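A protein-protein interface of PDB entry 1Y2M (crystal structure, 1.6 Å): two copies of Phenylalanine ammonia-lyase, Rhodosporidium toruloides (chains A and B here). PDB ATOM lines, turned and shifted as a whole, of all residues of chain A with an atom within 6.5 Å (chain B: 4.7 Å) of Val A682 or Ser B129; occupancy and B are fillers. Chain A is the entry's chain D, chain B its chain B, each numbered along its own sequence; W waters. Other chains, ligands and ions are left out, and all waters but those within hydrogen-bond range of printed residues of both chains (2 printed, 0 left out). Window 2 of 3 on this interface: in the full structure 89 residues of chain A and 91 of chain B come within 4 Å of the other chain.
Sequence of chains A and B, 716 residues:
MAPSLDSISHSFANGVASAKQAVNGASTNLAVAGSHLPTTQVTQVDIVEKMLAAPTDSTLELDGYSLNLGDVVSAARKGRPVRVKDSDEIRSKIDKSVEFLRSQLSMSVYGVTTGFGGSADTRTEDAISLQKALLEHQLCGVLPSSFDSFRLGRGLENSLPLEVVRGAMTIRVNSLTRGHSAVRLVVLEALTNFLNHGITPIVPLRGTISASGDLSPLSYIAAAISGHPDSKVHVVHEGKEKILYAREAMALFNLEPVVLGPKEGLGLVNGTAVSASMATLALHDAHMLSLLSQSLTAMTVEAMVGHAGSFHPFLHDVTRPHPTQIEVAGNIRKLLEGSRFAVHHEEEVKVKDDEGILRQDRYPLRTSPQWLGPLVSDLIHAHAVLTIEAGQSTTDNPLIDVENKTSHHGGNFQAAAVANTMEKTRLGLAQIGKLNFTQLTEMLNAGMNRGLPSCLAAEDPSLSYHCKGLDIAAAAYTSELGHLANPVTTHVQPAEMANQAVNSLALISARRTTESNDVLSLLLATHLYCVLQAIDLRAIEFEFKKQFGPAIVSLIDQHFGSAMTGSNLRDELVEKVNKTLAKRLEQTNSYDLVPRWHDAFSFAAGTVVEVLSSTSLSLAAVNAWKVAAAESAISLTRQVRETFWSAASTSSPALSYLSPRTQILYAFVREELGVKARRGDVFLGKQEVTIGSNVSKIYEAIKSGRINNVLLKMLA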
ATOM      1  N   LEU A 463     -15.534 -11.752 -24.344  1.00  0.00           N
ATOM      2  CA  LEU A 463     -16.249 -11.317 -23.161  1.00  0.00           C
ATOM      3  C   LEU A 463     -17.209 -12.369 -22.594  1.00  0.00           C
ATOM      4  O   LEU A 463     -18.137 -12.043 -21.843  1.00  0.00           O
ATOM      5  CB  LEU A 463     -16.979 -10.020 -23.464  1.00  0.00           C
ATOM      6  CG  LEU A 463     -15.996  -8.831 -23.587  1.00  0.00           C
ATOM      7  CD1 LEU A 463     -16.742  -7.583 -24.025  1.00  0.00           C
ATOM      8  CD2 LEU A 463     -15.246  -8.562 -22.284  1.00  0.00           C
ATOM      9  N   SER A 464     -16.928 -13.626 -22.891  1.00  0.00           N
ATOM     10  CA  SER A 464     -17.754 -14.711 -22.415  1.00  0.00           C
ATOM     11  C   SER A 464     -16.920 -15.982 -22.282  1.00  0.00           C
ATOM     12  O   SER A 464     -16.393 -16.509 -23.277  1.00  0.00           O
ATOM     13  CB  SER A 464     -18.893 -14.938 -23.379  1.00  0.00           C
ATOM     14  OG  SER A 464     -19.709 -15.988 -22.903  1.00  0.00           O
ATOM     15  N   GLY A 680     -25.164 -15.294 -22.591  1.00  0.00           N
ATOM     16  CA  GLY A 680     -23.993 -14.615 -22.058  1.00  0.00           C
ATOM     17  C   GLY A 680     -24.331 -13.271 -21.404  1.00  0.00           C
ATOM     18  O   GLY A 680     -25.011 -12.407 -21.996  1.00  0.00           O
ATOM     19  N   ASP A 681     -23.878 -13.090 -20.158  1.00  0.00           N
ATOM     20  CA  ASP A 681     -24.240 -11.896 -19.367  1.00  0.00           C
ATOM     21  C   ASP A 681     -23.817 -10.586 -20.051  1.00  0.00           C
ATOM     22  O   ASP A 681     -24.528  -9.596 -20.022  1.00  0.00           O
ATOM     23  CB  ASP A 681     -23.595 -11.916 -17.977  1.00  0.00           C
ATOM     24  CG  ASP A 681     -24.177 -12.941 -17.037  1.00  0.00           C
ATOM     25  OD1 ASP A 681     -25.140 -13.648 -17.406  1.00  0.00           O
ATOM     26  OD2 ASP A 681     -23.633 -12.996 -15.894  1.00  0.00           O
ATOM     27  N   VAL A 682     -22.624 -10.561 -20.640  1.00  0.00           N
ATOM     28  CA  VAL A 682     -22.151  -9.326 -21.259  1.00  0.00           C
ATOM     29  C   VAL A 682     -22.948  -8.999 -22.518  1.00  0.00           C
ATOM     30  O   VAL A 682     -23.395  -7.847 -22.702  1.00  0.00           O
ATOM     31  CB  VAL A 682     -20.615  -9.365 -21.534  1.00  0.00           C
ATOM     32  CG1 VAL A 682     -20.195  -8.111 -22.304  1.00  0.00           C
ATOM     33  CG2 VAL A 682     -19.812  -9.515 -20.218  1.00  0.00           C
ATOM     34  N   PHE A 683     -23.151 -10.005 -23.384  1.00  0.00           N
ATOM     35  CA  PHE A 683     -24.001  -9.811 -24.563  1.00  0.00           C
ATOM     36  C   PHE A 683     -25.348  -9.244 -24.196  1.00  0.00           C
ATOM     37  O   PHE A 683     -25.875  -8.303 -24.850  1.00  0.00           O
ATOM     38  CB  PHE A 683     -24.235 -11.093 -25.346  1.00  0.00           C
ATOM     39  CG  PHE A 683     -25.072 -10.867 -26.567  1.00  0.00           C
ATOM     40  CD1 PHE A 683     -24.479 -10.427 -27.751  1.00  0.00           C
ATOM     41  CD2 PHE A 683     -26.445 -11.018 -26.530  1.00  0.00           C
ATOM     42  CE1 PHE A 683     -25.253 -10.163 -28.865  1.00  0.00           C
ATOM     43  CE2 PHE A 683     -27.203 -10.751 -27.652  1.00  0.00           C
ATOM     44  CZ  PHE A 683     -26.608 -10.326 -28.805  1.00  0.00           C
ATOM     45  N   LEU A 684     -25.942  -9.857 -23.163  1.00  0.00           N
ATOM     46  CA  LEU A 684     -27.296  -9.483 -22.732  1.00  0.00           C
ATOM     47  C   LEU A 684     -27.387  -8.184 -21.926  1.00  0.00           C
ATOM     48  O   LEU A 684     -28.483  -7.653 -21.730  1.00  0.00           O
ATOM     49  CB  LEU A 684     -27.894 -10.603 -21.896  1.00  0.00           C
ATOM     50  CG  LEU A 684     -28.210 -11.904 -22.651  1.00  0.00           C
ATOM     51  CD1 LEU A 684     -28.542 -13.004 -21.641  1.00  0.00           C
ATOM     52  CD2 LEU A 684     -29.345 -11.694 -23.624  1.00  0.00           C
ATOM     53  N   GLY A 685     -26.264  -7.680 -21.445  1.00  0.00           N
ATOM     54  CA  GLY A 685     -26.285  -6.563 -20.516  1.00  0.00           C
ATOM     55  C   GLY A 685     -27.046  -6.883 -19.234  1.00  0.00           C
ATOM     56  O   GLY A 685     -27.580  -5.989 -18.590  1.00  0.00           O
ATOM     57  N   LYS A 686     -27.032  -8.153 -18.837  1.00  0.00           N
ATOM     58  CA  LYS A 686     -27.798  -8.624 -17.689  1.00  0.00           C
ATOM     59  C   LYS A 686     -26.998  -9.730 -17.000  1.00  0.00           C
ATOM     60  O   LYS A 686     -26.478 -10.630 -17.655  1.00  0.00           O
ATOM     61  CB  LYS A 686     -29.134  -9.202 -18.164  1.00  0.00           C
ATOM     62  CG  LYS A 686     -30.005  -9.770 -17.073  1.00  0.00           C
ATOM     63  CD  LYS A 686     -31.334 -10.357 -17.586  1.00  0.00           C
ATOM     64  CE  LYS A 686     -32.174 -10.891 -16.397  1.00  0.00           C
ATOM     65  NZ  LYS A 686     -33.606 -11.146 -16.847  1.00  0.00           N
ATOM     66  N   GLU B 125     -16.892   1.132 -19.355  1.00  0.00           N
ATOM     67  CA  GLU B 125     -17.988   0.183 -19.553  1.00  0.00           C
ATOM     68  C   GLU B 125     -17.423  -1.233 -19.760  1.00  0.00           C
ATOM     69  O   GLU B 125     -17.840  -2.181 -19.096  1.00  0.00           O
ATOM     70  CB  GLU B 125     -18.800   0.558 -20.803  1.00  0.00           C
ATOM     71  CG  GLU B 125     -19.449   1.952 -20.783  1.00  0.00           C
ATOM     72  CD  GLU B 125     -19.881   2.446 -22.186  1.00  0.00           C
ATOM     73  OE1 GLU B 125     -19.181   2.159 -23.192  1.00  0.00           O
ATOM     74  OE2 GLU B 125     -20.924   3.136 -22.270  1.00  0.00           O
ATOM     75  N   ASP B 126     -16.483  -1.364 -20.696  1.00  0.00           N
ATOM     76  CA  ASP B 126     -15.943  -2.679 -21.046  1.00  0.00           C
ATOM     77  C   ASP B 126     -15.185  -3.294 -19.870  1.00  0.00           C
ATOM     78  O   ASP B 126     -15.299  -4.487 -19.628  1.00  0.00           O
ATOM     79  CB  ASP B 126     -15.029  -2.589 -22.257  1.00  0.00           C
ATOM     80  CG  ASP B 126     -15.726  -1.986 -23.460  1.00  0.00           C
ATOM     81  OD1 ASP B 126     -16.950  -2.215 -23.603  1.00  0.00           O
ATOM     82  OD2 ASP B 126     -15.057  -1.276 -24.249  1.00  0.00           O
ATOM     83  N   ALA B 127     -14.410  -2.480 -19.147  1.00  0.00           N
ATOM     84  CA  ALA B 127     -13.767  -2.957 -17.905  1.00  0.00           C
ATOM     85  C   ALA B 127     -14.808  -3.463 -16.915  1.00  0.00           C
ATOM     86  O   ALA B 127     -14.594  -4.472 -16.242  1.00  0.00           O
ATOM     87  CB  ALA B 127     -12.915  -1.840 -17.257  1.00  0.00           C
ATOM     88  N   ILE B 128     -15.927  -2.749 -16.802  1.00  0.00           N
ATOM     89  CA  ILE B 128     -16.985  -3.184 -15.890  1.00  0.00           C
ATOM     90  C   ILE B 128     -17.525  -4.538 -16.401  1.00  0.00           C
ATOM     91  O   ILE B 128     -17.709  -5.467 -15.601  1.00  0.00           O
ATOM     92  CB  ILE B 128     -18.106  -2.100 -15.713  1.00  0.00           C
ATOM     93  CG1 ILE B 128     -17.589  -0.979 -14.794  1.00  0.00           C
ATOM     94  CG2 ILE B 128     -19.356  -2.693 -15.067  1.00  0.00           C
ATOM     95  CD1 ILE B 128     -18.409   0.321 -14.823  1.00  0.00           C
ATOM     96  N   SER B 129     -17.762  -4.623 -17.713  1.00  0.00           N
ATOM     97  CA  SER B 129     -18.214  -5.883 -18.360  1.00  0.00           C
ATOM     98  C   SER B 129     -17.251  -7.070 -18.191  1.00  0.00           C
ATOM     99  O   SER B 129     -17.681  -8.224 -18.012  1.00  0.00           O
ATOM    100  CB  SER B 129     -18.483  -5.664 -19.860  1.00  0.00           C
ATOM    101  OG  SER B 129     -19.639  -4.873 -20.064  1.00  0.00           O
ATOM    102  N   LEU B 130     -15.947  -6.803 -18.257  1.00  0.00           N
ATOM    103  CA  LEU B 130     -14.943  -7.859 -18.099  1.00  0.00           C
ATOM    104  C   LEU B 130     -15.036  -8.444 -16.715  1.00  0.00           C
ATOM    105  O   LEU B 130     -14.910  -9.663 -16.539  1.00  0.00           O
ATOM    106  CB  LEU B 130     -13.524  -7.303 -18.321  1.00  0.00           C
ATOM    107  CG  LEU B 130     -12.370  -8.298 -18.138  1.00  0.00           C
ATOM    108  CD1 LEU B 130     -12.549  -9.540 -19.000  1.00  0.00           C
ATOM    109  CD2 LEU B 130     -11.029  -7.604 -18.443  1.00  0.00           C
ATOM    110  N   GLN B 131     -15.223  -7.610 -15.695  1.00  0.00           N
ATOM    111  CA  GLN B 131     -15.275  -8.163 -14.347  1.00  0.00           C
ATOM    112  C   GLN B 131     -16.511  -9.064 -14.263  1.00  0.00           C
ATOM    113  O   GLN B 131     -16.497 -10.110 -13.617  1.00  0.00           O
ATOM    114  CB  GLN B 131     -15.333  -7.086 -13.243  1.00  0.00           C
ATOM    115  CG  GLN B 131     -14.352  -5.900 -13.351  1.00  0.00           C
ATOM    116  CD  GLN B 131     -12.971  -6.346 -13.762  1.00  0.00           C
ATOM    117  OE1 GLN B 131     -12.346  -7.178 -13.084  1.00  0.00           O
ATOM    118  NE2 GLN B 131     -12.485  -5.811 -14.874  1.00  0.00           N
ATOM    119  N   LYS B 132     -17.599  -8.620 -14.887  1.00  0.00           N
ATOM    120  CA  LYS B 132     -18.855  -9.398 -14.912  1.00  0.00           C
ATOM    121  C   LYS B 132     -18.675 -10.749 -15.632  1.00  0.00           C
ATOM    122  O   LYS B 132     -19.196 -11.781 -15.167  1.00  0.00           O
ATOM    123  CB  LYS B 132     -19.984  -8.582 -15.543  1.00  0.00           C
ATOM    124  CG  LYS B 132     -20.487  -7.456 -14.562  1.00  0.00           C
ATOM    125  CD  LYS B 132     -21.546  -6.563 -15.163  1.00  0.00           C
ATOM    126  CE  LYS B 132     -21.991  -5.468 -14.202  1.00  0.00           C
ATOM    127  NZ  LYS B 132     -23.009  -4.565 -14.852  1.00  0.00           N
ATOM    128  N   ALA B 133     -17.934 -10.762 -16.720  1.00  0.00           N
ATOM    129  CA  ALA B 133     -17.632 -12.069 -17.389  1.00  0.00           C
ATOM    130  C   ALA B 133     -16.779 -12.966 -16.514  1.00  0.00           C
ATOM    131  O   ALA B 133     -16.912 -14.182 -16.563  1.00  0.00           O
ATOM    132  CB  ALA B 133     -16.943 -11.879 -18.728  1.00  0.00           C
HETATM  133  O   HOH W   1     -25.196  -6.420 -16.104  1.00  0.00           O
HETATM  134  O   HOH W   2     -21.875 -11.679 -14.111  1.00  0.00           O
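Among the printed residues, pairs that only touch across the chains: Leu A463 with Ala B133 and Val A682 with Ser B129.
Water W2 bridges OD2 of Asp A681 and O of Lys B132.
Water W1 bridges NZ of Lys B132 (3.1 Å) and O of Gly A685 (3.5 Å).
The backbone carbonyl oxygen of Glu B125 is in hydrogen-bond range of the side-chain hydroxyl of Ser B129 (3.4 Å).
Hydrophobic or aromatic side chains of chain B that line the printed part of chain A: Ala B133.
Among the printed residues, 2 pairs touch across the chains.
Among the printed residues, no Asp or Glu carboxylate lies within 4 Å of a Lys or Arg side-chain nitrogen of the other chain.
Printed residues of chain B within 4 Å of Leu A463: Ala B133.
Printed residues of chain B within 4 Å of Val A682: Ser B129 (3.3 Å).
Glu B125 touches none of the printed residues of chain A.
Ser B129 touches one residue of chain A.
Of the printed residues of chain A, Ala B133 touches Leu A463.
The nearest printed residue of chain B that does not touch Val A682 is Ala B133 (4.005 Å).
The nearest residue of chain A that does not touch Ser B129 is Leu A463 (4.8 Å).
No position is printed for both chains.
Of the 2 pairs that touch across the chains among the printed residues, none has its exchanged pair printed and touching as well.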
